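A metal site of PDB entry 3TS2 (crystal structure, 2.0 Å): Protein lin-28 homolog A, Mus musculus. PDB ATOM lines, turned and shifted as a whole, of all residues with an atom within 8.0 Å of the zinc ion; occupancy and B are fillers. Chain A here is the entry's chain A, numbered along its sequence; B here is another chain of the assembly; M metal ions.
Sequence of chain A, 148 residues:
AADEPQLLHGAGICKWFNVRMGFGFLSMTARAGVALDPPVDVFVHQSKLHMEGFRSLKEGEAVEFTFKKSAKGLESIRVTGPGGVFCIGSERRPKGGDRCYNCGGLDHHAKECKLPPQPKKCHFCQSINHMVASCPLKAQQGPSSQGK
O of Cys 125 is in hydrogen-bond range of N of Ala 62 (2.8 Å). The side-chain sulfur (SG) of Cys 135 lies close to the backbone NH (N) of Lys 138. The backbone NH (N) of Cys 122 is in hydrogen-bond range of the backbone carbonyl oxygen (O) of Ser 127 (2.9 Å). The side-chain sulfur (SG) of Cys 122 lies close to the backbone NH (N) of Phe 124, 3.5 Å away. The side-chain hydroxyl (OG) of Ser 127 lies within hydrogen-bond range of a ring nitrogen (ND1) of His 130 (3.4 Å). The side-chain sulfur (SG) of Cys 135 lies close to the backbone NH (N) of Leu 137 (3.6 Å). The side-chain sulfur of Cys 125 lies close to the backbone NH of Ser 127 (3.6 Å).
Of the 23 residues printed, 4 come within 4 Å of the zinc ion.
The zinc ion is bound by NE2 of His 130, SG of Cys 125, SG of Cys 122 and SG of Cys 135. The zinc ion has four donor atoms within binding distance.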
ATOM      1  N   GLY A  60       4.577  -0.055  19.663  1.00  0.00           N
ATOM      2  CA  GLY A  60       3.737  -0.890  20.503  1.00  0.00           C
ATOM      3  C   GLY A  60       4.317  -2.179  21.036  1.00  0.00           C
ATOM      4  O   GLY A  60       3.672  -2.848  21.849  1.00  0.00           O
ATOM      5  N   GLU A  61       5.529  -2.566  20.601  1.00  0.00           N
ATOM      6  CA  GLU A  61       6.091  -3.803  21.104  1.00  0.00           C
ATOM      7  C   GLU A  61       6.424  -3.704  22.598  1.00  0.00           C
ATOM      8  O   GLU A  61       6.888  -2.665  23.079  1.00  0.00           O
ATOM      9  CB  GLU A  61       7.260  -4.358  20.246  1.00  0.00           C
ATOM     10  CG  GLU A  61       8.597  -3.622  20.378  1.00  0.00           C
ATOM     11  CD  GLU A  61       9.762  -4.326  19.682  1.00  0.00           C
ATOM     12  OE1 GLU A  61      10.117  -3.931  18.551  1.00  0.00           O
ATOM     13  OE2 GLU A  61      10.316  -5.267  20.282  1.00  0.00           O
ATOM     14  N   ALA A  62       6.177  -4.794  23.330  1.00  0.00           N
ATOM     15  CA  ALA A  62       6.391  -4.904  24.788  1.00  0.00           C
ATOM     16  C   ALA A  62       7.853  -4.892  25.150  1.00  0.00           C
ATOM     17  O   ALA A  62       8.646  -5.630  24.552  1.00  0.00           O
ATOM     18  CB  ALA A  62       5.723  -6.157  25.330  1.00  0.00           C
ATOM     19  N   LYS A 121       4.306 -15.451  24.032  1.00  0.00           N
ATOM     20  CA  LYS A 121       4.144 -14.014  23.879  1.00  0.00           C
ATOM     21  C   LYS A 121       3.409 -13.764  22.562  1.00  0.00           C
ATOM     22  O   LYS A 121       3.629 -14.491  21.578  1.00  0.00           O
ATOM     23  CB  LYS A 121       5.496 -13.300  23.839  1.00  0.00           C
ATOM     24  CG  LYS A 121       6.310 -13.436  25.167  1.00  0.00           C
ATOM     25  CD  LYS A 121       7.765 -12.984  25.058  1.00  0.00           C
ATOM     26  CE  LYS A 121       8.643 -13.872  24.171  1.00  0.00           C
ATOM     27  NZ  LYS A 121       9.001 -15.172  24.814  1.00  0.00           N
ATOM     28  N   CYS A 122       2.561 -12.737  22.545  1.00  0.00           N
ATOM     29  CA  CYS A 122       1.794 -12.320  21.376  1.00  0.00           C
ATOM     30  C   CYS A 122       2.731 -12.244  20.185  1.00  0.00           C
ATOM     31  O   CYS A 122       3.762 -11.547  20.249  1.00  0.00           O
ATOM     32  CB  CYS A 122       1.111 -10.981  21.625  1.00  0.00           C
ATOM     33  SG  CYS A 122       0.281 -10.307  20.163  1.00  0.00           S
ATOM     34  N   HIS A 123       2.413 -12.970  19.081  1.00  0.00           N
ATOM     35  CA  HIS A 123       3.254 -12.964  17.860  1.00  0.00           C
ATOM     36  C   HIS A 123       3.434 -11.551  17.274  1.00  0.00           C
ATOM     37  O   HIS A 123       4.473 -11.246  16.685  1.00  0.00           O
ATOM     38  CB  HIS A 123       2.674 -13.892  16.782  1.00  0.00           C
ATOM     39  CG  HIS A 123       2.731 -15.359  17.093  1.00  0.00           C
ATOM     40  ND1 HIS A 123       3.905 -15.962  17.543  1.00  0.00           N
ATOM     41  CD2 HIS A 123       1.788 -16.310  16.930  1.00  0.00           C
ATOM     42  CE1 HIS A 123       3.610 -17.238  17.691  1.00  0.00           C
ATOM     43  NE2 HIS A 123       2.351 -17.506  17.311  1.00  0.00           N
ATOM     44  N   PHE A 124       2.431 -10.697  17.464  1.00  0.00           N
ATOM     45  CA  PHE A 124       2.473  -9.343  16.940  1.00  0.00           C
ATOM     46  C   PHE A 124       3.233  -8.308  17.822  1.00  0.00           C
ATOM     47  O   PHE A 124       4.058  -7.551  17.275  1.00  0.00           O
ATOM     48  CB  PHE A 124       1.051  -8.829  16.618  1.00  0.00           C
ATOM     49  CG  PHE A 124       1.067  -7.593  15.749  1.00  0.00           C
ATOM     50  CD1 PHE A 124       1.287  -7.681  14.384  1.00  0.00           C
ATOM     51  CD2 PHE A 124       0.908  -6.332  16.312  1.00  0.00           C
ATOM     52  CE1 PHE A 124       1.314  -6.539  13.585  1.00  0.00           C
ATOM     53  CE2 PHE A 124       0.964  -5.187  15.505  1.00  0.00           C
ATOM     54  CZ  PHE A 124       1.147  -5.292  14.155  1.00  0.00           C
ATOM     55  N   CYS A 125       2.923  -8.234  19.129  1.00  0.00           N
ATOM     56  CA  CYS A 125       3.529  -7.196  19.977  1.00  0.00           C
ATOM     57  C   CYS A 125       4.437  -7.720  21.114  1.00  0.00           C
ATOM     58  O   CYS A 125       5.020  -6.907  21.841  1.00  0.00           O
ATOM     59  CB  CYS A 125       2.427  -6.277  20.513  1.00  0.00           C
ATOM     60  SG  CYS A 125       1.433  -7.020  21.840  1.00  0.00           S
ATOM     61  N   GLN A 126       4.521  -9.055  21.287  1.00  0.00           N
ATOM     62  CA  GLN A 126       5.309  -9.691  22.369  1.00  0.00           C
ATOM     63  C   GLN A 126       4.730  -9.559  23.787  1.00  0.00           C
ATOM     64  O   GLN A 126       5.396  -9.929  24.748  1.00  0.00           O
ATOM     65  CB  GLN A 126       6.846  -9.362  22.332  1.00  0.00           C
ATOM     66  CG  GLN A 126       7.619 -10.276  21.379  1.00  0.00           C
ATOM     67  CD  GLN A 126       9.116 -10.507  21.705  1.00  0.00           C
ATOM     68  OE1 GLN A 126       9.625 -11.624  21.509  1.00  0.00           O
ATOM     69  NE2 GLN A 126       9.936  -9.475  22.044  1.00  0.00           N
ATOM     70  N   SER A 127       3.475  -9.116  23.921  1.00  0.00           N
ATOM     71  CA  SER A 127       2.849  -9.054  25.244  1.00  0.00           C
ATOM     72  C   SER A 127       2.707 -10.450  25.861  1.00  0.00           C
ATOM     73  O   SER A 127       2.416 -11.436  25.166  1.00  0.00           O
ATOM     74  CB  SER A 127       1.491  -8.366  25.176  1.00  0.00           C
ATOM     75  OG  SER A 127       0.781  -8.547  26.390  1.00  0.00           O
ATOM     76  N   ILE A 128       2.920 -10.538  27.173  1.00  0.00           N
ATOM     77  CA  ILE A 128       2.732 -11.813  27.872  1.00  0.00           C
ATOM     78  C   ILE A 128       1.294 -11.969  28.317  1.00  0.00           C
ATOM     79  O   ILE A 128       0.901 -13.060  28.737  1.00  0.00           O
ATOM     80  CB  ILE A 128       3.763 -12.149  28.990  1.00  0.00           C
ATOM     81  CG1 ILE A 128       3.991 -11.039  30.062  1.00  0.00           C
ATOM     82  CG2 ILE A 128       5.102 -12.474  28.341  1.00  0.00           C
ATOM     83  CD1 ILE A 128       2.837 -10.411  30.852  1.00  0.00           C
ATOM     84  N   ASN A 129       0.511 -10.875  28.246  1.00  0.00           N
ATOM     85  CA  ASN A 129      -0.873 -10.795  28.694  1.00  0.00           C
ATOM     86  C   ASN A 129      -1.947 -11.232  27.717  1.00  0.00           C
ATOM     87  O   ASN A 129      -3.090 -11.423  28.144  1.00  0.00           O
ATOM     88  CB  ASN A 129      -1.185  -9.419  29.305  1.00  0.00           C
ATOM     89  CG  ASN A 129      -0.494  -9.130  30.609  1.00  0.00           C
ATOM     90  OD1 ASN A 129      -0.433  -9.957  31.521  1.00  0.00           O
ATOM     91  ND2 ASN A 129       0.039  -7.955  30.726  1.00  0.00           N
ATOM     92  N   HIS A 130      -1.614 -11.417  26.429  1.00  0.00           N
ATOM     93  CA  HIS A 130      -2.577 -11.874  25.418  1.00  0.00           C
ATOM     94  C   HIS A 130      -1.864 -12.598  24.273  1.00  0.00           C
ATOM     95  O   HIS A 130      -0.645 -12.488  24.118  1.00  0.00           O
ATOM     96  CB  HIS A 130      -3.425 -10.683  24.867  1.00  0.00           C
ATOM     97  CG  HIS A 130      -2.627  -9.664  24.124  1.00  0.00           C
ATOM     98  ND1 HIS A 130      -2.213  -8.494  24.732  1.00  0.00           N
ATOM     99  CD2 HIS A 130      -2.187  -9.675  22.842  1.00  0.00           C
ATOM    100  CE1 HIS A 130      -1.544  -7.828  23.807  1.00  0.00           C
ATOM    101  NE2 HIS A 130      -1.485  -8.506  22.652  1.00  0.00           N
ATOM    102  N   MET A 131      -2.657 -13.312  23.452  1.00  0.00           N
ATOM    103  CA  MET A 131      -2.166 -13.980  22.262  1.00  0.00           C
ATOM    104  C   MET A 131      -2.626 -13.178  21.052  1.00  0.00           C
ATOM    105  O   MET A 131      -3.486 -12.300  21.215  1.00  0.00           O
ATOM    106  CB  MET A 131      -2.606 -15.444  22.227  1.00  0.00           C
ATOM    107  CG  MET A 131      -1.918 -16.256  23.318  1.00  0.00           C
ATOM    108  SD  MET A 131      -1.952 -18.006  22.975  1.00  0.00           S
ATOM    109  CE  MET A 131      -3.415 -18.484  23.879  1.00  0.00           C
ATOM    110  N   VAL A 132      -2.017 -13.402  19.860  1.00  0.00           N
ATOM    111  CA  VAL A 132      -2.240 -12.630  18.636  1.00  0.00           C
ATOM    112  C   VAL A 132      -3.726 -12.456  18.190  1.00  0.00           C
ATOM    113  O   VAL A 132      -4.098 -11.368  17.757  1.00  0.00           O
ATOM    114  CB  VAL A 132      -1.233 -12.966  17.500  1.00  0.00           C
ATOM    115  CG1 VAL A 132      -1.499 -14.336  16.883  1.00  0.00           C
ATOM    116  CG2 VAL A 132      -1.193 -11.867  16.436  1.00  0.00           C
ATOM    117  N   ALA A 133      -4.567 -13.486  18.347  1.00  0.00           N
ATOM    118  CA  ALA A 133      -5.988 -13.424  17.964  1.00  0.00           C
ATOM    119  C   ALA A 133      -6.769 -12.349  18.738  1.00  0.00           C
ATOM    120  O   ALA A 133      -7.814 -11.899  18.282  1.00  0.00           O
ATOM    121  CB  ALA A 133      -6.657 -14.783  18.152  1.00  0.00           C
ATOM    122  N   SER A 134      -6.242 -11.927  19.894  1.00  0.00           N
ATOM    123  CA  SER A 134      -6.853 -10.904  20.755  1.00  0.00           C
ATOM    124  C   SER A 134      -5.969  -9.657  20.887  1.00  0.00           C
ATOM    125  O   SER A 134      -6.182  -8.871  21.809  1.00  0.00           O
ATOM    126  CB  SER A 134      -7.151 -11.488  22.133  1.00  0.00           C
ATOM    127  OG  SER A 134      -8.076 -12.555  22.076  1.00  0.00           O
ATOM    128  N   CYS A 135      -4.985  -9.480  19.972  1.00  0.00           N
ATOM    129  CA  CYS A 135      -4.053  -8.341  20.024  1.00  0.00           C
ATOM    130  C   CYS A 135      -4.745  -6.998  19.728  1.00  0.00           C
ATOM    131  O   CYS A 135      -5.182  -6.777  18.598  1.00  0.00           O
ATOM    132  CB  CYS A 135      -2.834  -8.547  19.114  1.00  0.00           C
ATOM    133  SG  CYS A 135      -1.586  -7.244  19.257  1.00  0.00           S
ATOM    134  N   PRO A 136      -4.804  -6.059  20.713  1.00  0.00           N
ATOM    135  CA  PRO A 136      -5.427  -4.742  20.441  1.00  0.00           C
ATOM    136  C   PRO A 136      -4.604  -3.859  19.503  1.00  0.00           C
ATOM    137  O   PRO A 136      -5.159  -3.007  18.820  1.00  0.00           O
ATOM    138  CB  PRO A 136      -5.554  -4.122  21.840  1.00  0.00           C
ATOM    139  CG  PRO A 136      -4.459  -4.763  22.653  1.00  0.00           C
ATOM    140  CD  PRO A 136      -4.300  -6.158  22.107  1.00  0.00           C
ATOM    141  N   LEU A 137      -3.279  -4.083  19.459  1.00  0.00           N
ATOM    142  CA  LEU A 137      -2.368  -3.346  18.583  1.00  0.00           C
ATOM    143  C   LEU A 137      -2.558  -3.767  17.118  1.00  0.00           C
ATOM    144  O   LEU A 137      -2.565  -2.905  16.234  1.00  0.00           O
ATOM    145  CB  LEU A 137      -0.916  -3.523  19.046  1.00  0.00           C
ATOM    146  CG  LEU A 137       0.139  -2.705  18.293  1.00  0.00           C
ATOM    147  CD1 LEU A 137       0.066  -1.196  18.639  1.00  0.00           C
ATOM    148  CD2 LEU A 137       1.530  -3.253  18.541  1.00  0.00           C
ATOM    149  N   LYS A 138      -2.709  -5.081  16.877  1.00  0.00           N
ATOM    150  CA  LYS A 138      -2.930  -5.639  15.536  1.00  0.00           C
ATOM    151  C   LYS A 138      -4.301  -5.197  14.991  1.00  0.00           C
ATOM    152  O   LYS A 138      -4.439  -5.024  13.777  1.00  0.00           O
ATOM    153  CB  LYS A 138      -2.803  -7.173  15.555  1.00  0.00           C
ATOM    154  CG  LYS A 138      -2.684  -7.815  14.174  1.00  0.00           C
ATOM    155  CD  LYS A 138      -2.869  -9.316  14.246  1.00  0.00           C
ATOM    156  CE  LYS A 138      -3.012  -9.985  12.897  1.00  0.00           C
ATOM    157  NZ  LYS A 138      -1.720 -10.129  12.185  1.00  0.00           N
ATOM    158  N   ALA A 139      -5.311  -4.986  15.896  1.00  0.00           N
ATOM    159  CA  ALA A 139      -6.679  -4.557  15.531  1.00  0.00           C
ATOM    160  C   ALA A 139      -6.739  -3.366  14.543  1.00  0.00           C
ATOM    161  O   ALA A 139      -7.612  -3.360  13.675  1.00  0.00           O
ATOM    162  CB  ALA A 139      -7.492  -4.266  16.778  1.00  0.00           C
ATOM    163  P     G B  21      -4.021 -22.268  17.531  1.00  0.00           P
ATOM    164  OP1   G B  21      -4.409 -23.586  18.047  1.00  0.00           O
ATOM    165  OP2   G B  21      -4.820 -21.099  18.007  1.00  0.00           O
ATOM    166  O5'   G B  21      -2.475 -21.994  17.834  1.00  0.00           O
ATOM    167  C5'   G B  21      -1.477 -23.015  17.782  1.00  0.00           C
ATOM    168  C4'   G B  21      -0.561 -22.862  18.982  1.00  0.00           C
ATOM    169  O4'   G B  21      -0.016 -21.516  18.966  1.00  0.00           O
ATOM    170  C3'   G B  21      -1.219 -23.027  20.348  1.00  0.00           C
ATOM    171  O3'   G B  21      -0.323 -23.700  21.225  1.00  0.00           O
ATOM    172  C2'   G B  21      -1.466 -21.602  20.826  1.00  0.00           C
ATOM    173  O2'   G B  21      -1.540 -21.463  22.224  1.00  0.00           O
ATOM    174  C1'   G B  21      -0.245 -20.904  20.223  1.00  0.00           C
ATOM    175  N9    G B  21      -0.414 -19.476  19.998  1.00  0.00           N
ATOM    176  C8    G B  21      -1.498 -18.808  19.473  1.00  0.00           C
ATOM    177  N7    G B  21      -1.325 -17.518  19.364  1.00  0.00           N
ATOM    178  C5    G B  21      -0.043 -17.316  19.854  1.00  0.00           C
ATOM    179  C6    G B  21       0.692 -16.111  20.043  1.00  0.00           C
ATOM    180  O6    G B  21       0.360 -14.967  19.712  1.00  0.00           O
ATOM    181  N1    G B  21       1.994 -16.347  20.493  1.00  0.00           N
ATOM    182  C2    G B  21       2.486 -17.596  20.802  1.00  0.00           C
ATOM    183  N2    G B  21       3.733 -17.630  21.254  1.00  0.00           N
ATOM    184  N3    G B  21       1.800 -18.727  20.675  1.00  0.00           N
ATOM    185  C4    G B  21       0.547 -18.519  20.193  1.00  0.00           C
HETATM  186 ZN    ZN M   1      -0.323  -8.203  20.989  1.00  0.00          ZN
